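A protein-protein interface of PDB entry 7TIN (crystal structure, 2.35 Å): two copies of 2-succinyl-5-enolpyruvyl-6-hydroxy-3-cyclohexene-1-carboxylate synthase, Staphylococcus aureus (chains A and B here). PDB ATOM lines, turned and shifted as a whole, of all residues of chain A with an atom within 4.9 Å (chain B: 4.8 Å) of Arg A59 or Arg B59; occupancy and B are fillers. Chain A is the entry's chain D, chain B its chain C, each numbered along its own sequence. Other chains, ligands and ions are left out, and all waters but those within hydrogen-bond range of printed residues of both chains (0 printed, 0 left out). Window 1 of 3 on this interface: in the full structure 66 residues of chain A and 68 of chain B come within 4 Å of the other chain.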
ATOM      1  N   ASP A  57      -8.978  28.359  -1.454  1.00  0.00           N
ATOM      2  CA  ASP A  57     -10.313  27.773  -1.376  1.00  0.00           C
ATOM      3  C   ASP A  57     -11.196  28.444  -2.424  1.00  0.00           C
ATOM      4  O   ASP A  57     -11.566  29.614  -2.276  1.00  0.00           O
ATOM      5  CB  ASP A  57     -10.908  27.922   0.025  1.00  0.00           C
ATOM      6  CG  ASP A  57     -12.139  27.049   0.231  1.00  0.00           C
ATOM      7  OD1 ASP A  57     -12.768  26.658  -0.777  1.00  0.00           O
ATOM      8  OD2 ASP A  57     -12.483  26.752   1.400  1.00  0.00           O
ATOM      9  N   GLU A  58     -11.542  27.688  -3.473  1.00  0.00           N
ATOM     10  CA  GLU A  58     -12.292  28.253  -4.593  1.00  0.00           C
ATOM     11  C   GLU A  58     -13.669  28.747  -4.171  1.00  0.00           C
ATOM     12  O   GLU A  58     -14.158  29.745  -4.713  1.00  0.00           O
ATOM     13  CB  GLU A  58     -12.423  27.214  -5.714  1.00  0.00           C
ATOM     14  CG  GLU A  58     -11.182  27.065  -6.574  1.00  0.00           C
ATOM     15  CD  GLU A  58     -10.245  25.986  -6.062  1.00  0.00           C
ATOM     16  OE1 GLU A  58     -10.559  25.361  -5.027  1.00  0.00           O
ATOM     17  OE2 GLU A  58      -9.193  25.765  -6.692  1.00  0.00           O
ATOM     18  N   ARG A  59     -14.316  28.065  -3.221  1.00  0.00           N
ATOM     19  CA  ARG A  59     -15.640  28.500  -2.782  1.00  0.00           C
ATOM     20  C   ARG A  59     -15.578  29.863  -2.107  1.00  0.00           C
ATOM     21  O   ARG A  59     -16.440  30.719  -2.341  1.00  0.00           O
ATOM     22  CB  ARG A  59     -16.259  27.472  -1.835  1.00  0.00           C
ATOM     23  CG  ARG A  59     -17.663  27.856  -1.377  1.00  0.00           C
ATOM     24  CD  ARG A  59     -18.289  26.805  -0.480  1.00  0.00           C
ATOM     25  NE  ARG A  59     -17.602  26.694   0.800  1.00  0.00           N
ATOM     26  CZ  ARG A  59     -18.072  26.031   1.847  1.00  0.00           C
ATOM     27  NH1 ARG A  59     -19.238  25.408   1.804  1.00  0.00           N
ATOM     28  NH2 ARG A  59     -17.356  25.997   2.969  1.00  0.00           N
ATOM     29  N   SER A  60     -14.570  30.078  -1.258  1.00  0.00           N
ATOM     30  CA  SER A  60     -14.412  31.375  -0.615  1.00  0.00           C
ATOM     31  C   SER A  60     -13.907  32.420  -1.598  1.00  0.00           C
ATOM     32  O   SER A  60     -14.305  33.588  -1.519  1.00  0.00           O
ATOM     33  CB  SER A  60     -13.463  31.255   0.577  1.00  0.00           C
ATOM     34  OG  SER A  60     -14.084  30.594   1.666  1.00  0.00           O
ATOM     35  N   ALA A  61     -13.042  32.016  -2.533  1.00  0.00           N
ATOM     36  CA  ALA A  61     -12.503  32.955  -3.510  1.00  0.00           C
ATOM     37  C   ALA A  61     -13.613  33.591  -4.335  1.00  0.00           C
ATOM     38  O   ALA A  61     -13.607  34.806  -4.570  1.00  0.00           O
ATOM     39  CB  ALA A  61     -11.504  32.247  -4.418  1.00  0.00           C
ATOM     40  N   ALA A  62     -14.579  32.786  -4.780  1.00  0.00           N
ATOM     41  CA  ALA A  62     -15.666  33.326  -5.587  1.00  0.00           C
ATOM     42  C   ALA A  62     -16.521  34.298  -4.783  1.00  0.00           C
ATOM     43  O   ALA A  62     -16.963  35.325  -5.309  1.00  0.00           O
ATOM     44  CB  ALA A  62     -16.510  32.185  -6.153  1.00  0.00           C
ATOM     45  N   PHE A  63     -16.758  34.001  -3.505  1.00  0.00           N
ATOM     46  CA  PHE A  63     -17.500  34.929  -2.655  1.00  0.00           C
ATOM     47  C   PHE A  63     -16.669  36.171  -2.352  1.00  0.00           C
ATOM     48  O   PHE A  63     -17.209  37.279  -2.245  1.00  0.00           O
ATOM     49  CB  PHE A  63     -17.917  34.234  -1.360  1.00  0.00           C
ATOM     50  CG  PHE A  63     -19.207  33.462  -1.466  1.00  0.00           C
ATOM     51  CD1 PHE A  63     -20.408  34.115  -1.711  1.00  0.00           C
ATOM     52  CD2 PHE A  63     -19.218  32.078  -1.320  1.00  0.00           C
ATOM     53  CE1 PHE A  63     -21.601  33.407  -1.799  1.00  0.00           C
ATOM     54  CE2 PHE A  63     -20.407  31.360  -1.406  1.00  0.00           C
ATOM     55  CZ  PHE A  63     -21.600  32.026  -1.646  1.00  0.00           C
ATOM     56  N   ASN A  88     -16.599  24.307  -7.122  1.00  0.00           N
ATOM     57  CA  ASN A  88     -16.707  25.085  -5.893  1.00  0.00           C
ATOM     58  C   ASN A  88     -17.219  26.505  -6.137  1.00  0.00           C
ATOM     59  O   ASN A  88     -17.627  27.173  -5.181  1.00  0.00           O
ATOM     60  CB  ASN A  88     -15.353  25.128  -5.178  1.00  0.00           C
ATOM     61  CG  ASN A  88     -15.036  23.838  -4.435  1.00  0.00           C
ATOM     62  OD1 ASN A  88     -15.344  23.697  -3.252  1.00  0.00           O
ATOM     63  ND2 ASN A  88     -14.415  22.893  -5.129  1.00  0.00           N
ATOM     64  N   PRO A  91     -21.965  27.933  -5.693  1.00  0.00           N
ATOM     65  CA  PRO A  91     -22.790  28.733  -4.764  1.00  0.00           C
ATOM     66  C   PRO A  91     -22.694  30.233  -4.996  1.00  0.00           C
ATOM     67  O   PRO A  91     -23.725  30.922  -4.989  1.00  0.00           O
ATOM     68  CB  PRO A  91     -22.261  28.345  -3.372  1.00  0.00           C
ATOM     69  CG  PRO A  91     -21.141  27.406  -3.579  1.00  0.00           C
ATOM     70  CD  PRO A  91     -21.123  26.948  -4.990  1.00  0.00           C
ATOM     71  N   HIS A 445     -19.544  28.328   8.645  1.00  0.00           N
ATOM     72  CA  HIS A 445     -19.691  27.925   7.248  1.00  0.00           C
ATOM     73  C   HIS A 445     -18.552  28.466   6.388  1.00  0.00           C
ATOM     74  O   HIS A 445     -17.968  27.732   5.583  1.00  0.00           O
ATOM     75  CB  HIS A 445     -21.047  28.394   6.714  1.00  0.00           C
ATOM     76  CG  HIS A 445     -21.641  27.482   5.683  1.00  0.00           C
ATOM     77  ND1 HIS A 445     -21.153  27.394   4.395  1.00  0.00           N
ATOM     78  CD2 HIS A 445     -22.685  26.620   5.749  1.00  0.00           C
ATOM     79  CE1 HIS A 445     -21.871  26.517   3.715  1.00  0.00           C
ATOM     80  NE2 HIS A 445     -22.806  26.033   4.514  1.00  0.00           N
ATOM     81  N   ASN A 448     -13.101  29.342   6.419  1.00  0.00           N
ATOM     82  CA  ASN A 448     -11.942  29.406   5.533  1.00  0.00           C
ATOM     83  C   ASN A 448     -11.735  30.796   4.945  1.00  0.00           C
ATOM     84  O   ASN A 448     -10.606  31.137   4.575  1.00  0.00           O
ATOM     85  CB  ASN A 448     -12.080  28.407   4.385  1.00  0.00           C
ATOM     86  CG  ASN A 448     -11.632  27.012   4.760  1.00  0.00           C
ATOM     87  OD1 ASN A 448     -11.368  26.722   5.928  1.00  0.00           O
ATOM     88  ND2 ASN A 448     -11.533  26.137   3.762  1.00  0.00           N
ATOM     89  N   ASP B  57     -22.459  22.312   7.188  1.00  0.00           N
ATOM     90  CA  ASP B  57     -21.780  22.699   5.951  1.00  0.00           C
ATOM     91  C   ASP B  57     -22.149  21.713   4.843  1.00  0.00           C
ATOM     92  O   ASP B  57     -21.748  20.545   4.880  1.00  0.00           O
ATOM     93  CB  ASP B  57     -20.266  22.764   6.149  1.00  0.00           C
ATOM     94  CG  ASP B  57     -19.544  23.409   4.970  1.00  0.00           C
ATOM     95  OD1 ASP B  57     -20.132  23.487   3.869  1.00  0.00           O
ATOM     96  OD2 ASP B  57     -18.385  23.841   5.140  1.00  0.00           O
ATOM     97  N   GLU B  58     -22.887  22.201   3.841  1.00  0.00           N
ATOM     98  CA  GLU B  58     -23.374  21.324   2.781  1.00  0.00           C
ATOM     99  C   GLU B  58     -22.232  20.754   1.949  1.00  0.00           C
ATOM    100  O   GLU B  58     -22.300  19.600   1.505  1.00  0.00           O
ATOM    101  CB  GLU B  58     -24.360  22.080   1.891  1.00  0.00           C
ATOM    102  CG  GLU B  58     -25.735  22.268   2.514  1.00  0.00           C
ATOM    103  CD  GLU B  58     -25.832  23.517   3.375  1.00  0.00           C
ATOM    104  OE1 GLU B  58     -24.852  24.291   3.432  1.00  0.00           O
ATOM    105  OE2 GLU B  58     -26.894  23.723   3.999  1.00  0.00           O
ATOM    106  N   ARG B  59     -21.175  21.537   1.720  1.00  0.00           N
ATOM    107  CA  ARG B  59     -20.050  21.022   0.944  1.00  0.00           C
ATOM    108  C   ARG B  59     -19.391  19.846   1.654  1.00  0.00           C
ATOM    109  O   ARG B  59     -19.169  18.786   1.053  1.00  0.00           O
ATOM    110  CB  ARG B  59     -19.027  22.126   0.683  1.00  0.00           C
ATOM    111  CG  ARG B  59     -17.842  21.637  -0.145  1.00  0.00           C
ATOM    112  CD  ARG B  59     -16.912  22.769  -0.543  1.00  0.00           C
ATOM    113  NE  ARG B  59     -16.173  23.295   0.598  1.00  0.00           N
ATOM    114  CZ  ARG B  59     -15.097  24.066   0.506  1.00  0.00           C
ATOM    115  NH1 ARG B  59     -14.593  24.414  -0.666  1.00  0.00           N
ATOM    116  NH2 ARG B  59     -14.517  24.506   1.621  1.00  0.00           N
ATOM    117  N   SER B  60     -19.084  20.010   2.943  1.00  0.00           N
ATOM    118  CA  SER B  60     -18.431  18.937   3.683  1.00  0.00           C
ATOM    119  C   SER B  60     -19.378  17.775   3.948  1.00  0.00           C
ATOM    120  O   SER B  60     -18.934  16.624   4.015  1.00  0.00           O
ATOM    121  CB  SER B  60     -17.865  19.473   4.995  1.00  0.00           C
ATOM    122  OG  SER B  60     -16.613  20.099   4.782  1.00  0.00           O
ATOM    123  N   ALA B  61     -20.677  18.051   4.087  1.00  0.00           N
ATOM    124  CA  ALA B  61     -21.640  16.982   4.330  1.00  0.00           C
ATOM    125  C   ALA B  61     -21.657  15.979   3.183  1.00  0.00           C
ATOM    126  O   ALA B  61     -21.662  14.763   3.410  1.00  0.00           O
ATOM    127  CB  ALA B  61     -23.033  17.574   4.545  1.00  0.00           C
ATOM    128  N   ALA B  62     -21.649  16.471   1.943  1.00  0.00           N
ATOM    129  CA  ALA B  62     -21.713  15.576   0.793  1.00  0.00           C
ATOM    130  C   ALA B  62     -20.450  14.725   0.677  1.00  0.00           C
ATOM    131  O   ALA B  62     -20.529  13.537   0.339  1.00  0.00           O
ATOM    132  CB  ALA B  62     -21.949  16.388  -0.482  1.00  0.00           C
ATOM    133  N   PHE B  63     -19.278  15.310   0.952  1.00  0.00           N
ATOM    134  CA  PHE B  63     -18.043  14.528   0.945  1.00  0.00           C
ATOM    135  C   PHE B  63     -18.023  13.523   2.092  1.00  0.00           C
ATOM    136  O   PHE B  63     -17.483  12.419   1.951  1.00  0.00           O
ATOM    137  CB  PHE B  63     -16.827  15.451   1.035  1.00  0.00           C
ATOM    138  CG  PHE B  63     -16.356  15.982  -0.293  1.00  0.00           C
ATOM    139  CD1 PHE B  63     -15.827  15.133  -1.250  1.00  0.00           C
ATOM    140  CD2 PHE B  63     -16.418  17.339  -0.572  1.00  0.00           C
ATOM    141  CE1 PHE B  63     -15.381  15.625  -2.464  1.00  0.00           C
ATOM    142  CE2 PHE B  63     -15.971  17.836  -1.782  1.00  0.00           C
ATOM    143  CZ  PHE B  63     -15.453  16.977  -2.731  1.00  0.00           C
ATOM    144  N   ASN B  88     -23.853  23.814  -3.005  1.00  0.00           N
ATOM    145  CA  ASN B  88     -22.648  23.393  -2.304  1.00  0.00           C
ATOM    146  C   ASN B  88     -22.358  21.911  -2.479  1.00  0.00           C
ATOM    147  O   ASN B  88     -21.255  21.467  -2.138  1.00  0.00           O
ATOM    148  CB  ASN B  88     -22.768  23.726  -0.815  1.00  0.00           C
ATOM    149  CG  ASN B  88     -22.449  25.177  -0.514  1.00  0.00           C
ATOM    150  OD1 ASN B  88     -21.313  25.517  -0.192  1.00  0.00           O
ATOM    151  ND2 ASN B  88     -23.452  26.042  -0.620  1.00  0.00           N
ATOM    152  N   PRO B  91     -19.253  19.915  -5.797  1.00  0.00           N
ATOM    153  CA  PRO B  91     -17.913  19.294  -5.803  1.00  0.00           C
ATOM    154  C   PRO B  91     -17.931  17.801  -5.510  1.00  0.00           C
ATOM    155  O   PRO B  91     -17.286  17.027  -6.230  1.00  0.00           O
ATOM    156  CB  PRO B  91     -17.161  20.088  -4.725  1.00  0.00           C
ATOM    157  CG  PRO B  91     -17.825  21.415  -4.731  1.00  0.00           C
ATOM    158  CD  PRO B  91     -19.283  21.107  -4.929  1.00  0.00           C
ATOM    159  N   HIS B 445      -8.350  23.213   3.100  1.00  0.00           N
ATOM    160  CA  HIS B 445      -9.507  23.234   2.212  1.00  0.00           C
ATOM    161  C   HIS B 445     -10.752  22.684   2.897  1.00  0.00           C
ATOM    162  O   HIS B 445     -11.836  23.270   2.787  1.00  0.00           O
ATOM    163  CB  HIS B 445      -9.201  22.442   0.941  1.00  0.00           C
ATOM    164  CG  HIS B 445      -9.827  23.009  -0.295  1.00  0.00           C
ATOM    165  ND1 HIS B 445     -11.188  22.983  -0.522  1.00  0.00           N
ATOM    166  CD2 HIS B 445      -9.275  23.603  -1.381  1.00  0.00           C
ATOM    167  CE1 HIS B 445     -11.448  23.544  -1.690  1.00  0.00           C
ATOM    168  NE2 HIS B 445     -10.304  23.926  -2.233  1.00  0.00           N
ATOM    169  N   ASN B 448     -13.418  22.610   7.754  1.00  0.00           N
ATOM    170  CA  ASN B 448     -14.788  22.498   8.239  1.00  0.00           C
ATOM    171  C   ASN B 448     -15.227  21.051   8.434  1.00  0.00           C
ATOM    172  O   ASN B 448     -16.147  20.798   9.219  1.00  0.00           O
ATOM    173  CB  ASN B 448     -15.748  23.192   7.268  1.00  0.00           C
ATOM    174  CG  ASN B 448     -15.853  24.686   7.513  1.00  0.00           C
ATOM    175  OD1 ASN B 448     -14.901  25.322   7.970  1.00  0.00           O
ATOM    176  ND2 ASN B 448     -17.016  25.256   7.204  1.00  0.00           N
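Among the printed residues, pairs that only touch across the chains: His A445 with Asp B57 (3.5 Å), Asp A57 with His B445 (3.5 Å), Asn A88 with Pro B91 (3.7 Å) and Pro A91 with Asn B88 (3.8 Å).
OD1 of Asp B57 is in salt-bridge range of NH1 of Arg A59 (3.0 Å).
The side-chain carboxylate of Glu B58 sits at hydrogen-bond distance from a ring nitrogen (NE2) of His A445, at 2.9 Å.
NH1 of Arg B59 lies within salt-bridge range of OD1 of Asp A57 (2.9 Å).
NH1 of Arg B59 is in hydrogen-bond range of OD1 of Asn A88 (2.8 Å).
The guanidinium group (NH1) of Arg A59 lies within hydrogen-bond range of the side-chain amide oxygen (OD1) of Asn B88.
A ring nitrogen (NE2) of His B445 is in hydrogen-bond range of the side-chain carboxylate (OE1) of Glu A58.
The side-chain amide nitrogen (ND2) of Asn A448 is in hydrogen-bond range of the backbone carbonyl oxygen (O) of His B445.
ND2 of Asn B448 lies within hydrogen-bond range of O of His A445 (3.1 Å).
NH2 of Arg A59 lies close to NH2 of Arg B59, at 3.5 Å.
Asp A57 touches His B445, and with the chains exchanged His A445 touches Asp B57.
Glu A58 touches His B445, and with the chains exchanged His A445 touches Glu B58.
Arg A59 touches Asn B88, and with the chains exchanged Asn A88 touches Arg B59.
His A445 touches Asn B448, and with the chains exchanged Asn A448 touches His B445.
11 positions are printed for both chains.
Of chain B, only Asp B57, Arg B59 and Asn B88 come within 4 Å of Arg A59.
Of the printed residues of chain A, Arg B59 touches Asp A57, Arg A59 and Asn A88.
Printed residues of chain A within 4 Å of Pro B91: Asn A88.
Printed residues of chain A within 4 Å of Asp B57: Arg A59 (3.0 Å) and His A445 (3.5 Å).
Ala B62 touches none of the printed residues of chain A.
The nearest printed residue of chain A that does not touch Arg B59 is Asn A448 (4.02 Å).
The nearest printed residue of chain B that does not touch His A445 is Asn B88 (4.1 Å).
Of the 11 printed residues of chain A, 7 touch a printed residue of chain B.
Hydrophobic or aromatic side chains of chain A within 4 Å of the printed part of chain B: Pro A91 and His A445.
Among the printed residues, 13 pairs touch across the chains.
The side-chain carboxylate (OD1) of Asp B57 is in hydrogen-bond range of the backbone NH (N) of Arg B59 (3.1 Å).
OD2 of Asp B57 lies within hydrogen-bond range of ND2 of Asn B448 (2.9 Å).
The guanidinium group of Arg B59 lies within hydrogen-bond range of the backbone carbonyl oxygen of His B445.
The side-chain carboxylate of Asp A57 is in hydrogen-bond range of the backbone NH of Arg A59, 3.2 Å away.
The side-chain amide nitrogen of Asn A448 is in hydrogen-bond range of the side-chain carboxylate of Asp A57 (2.6 Å).
The guanidinium group of Arg A59 sits at hydrogen-bond distance from the backbone carbonyl oxygen of His A445 (3.2 Å).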
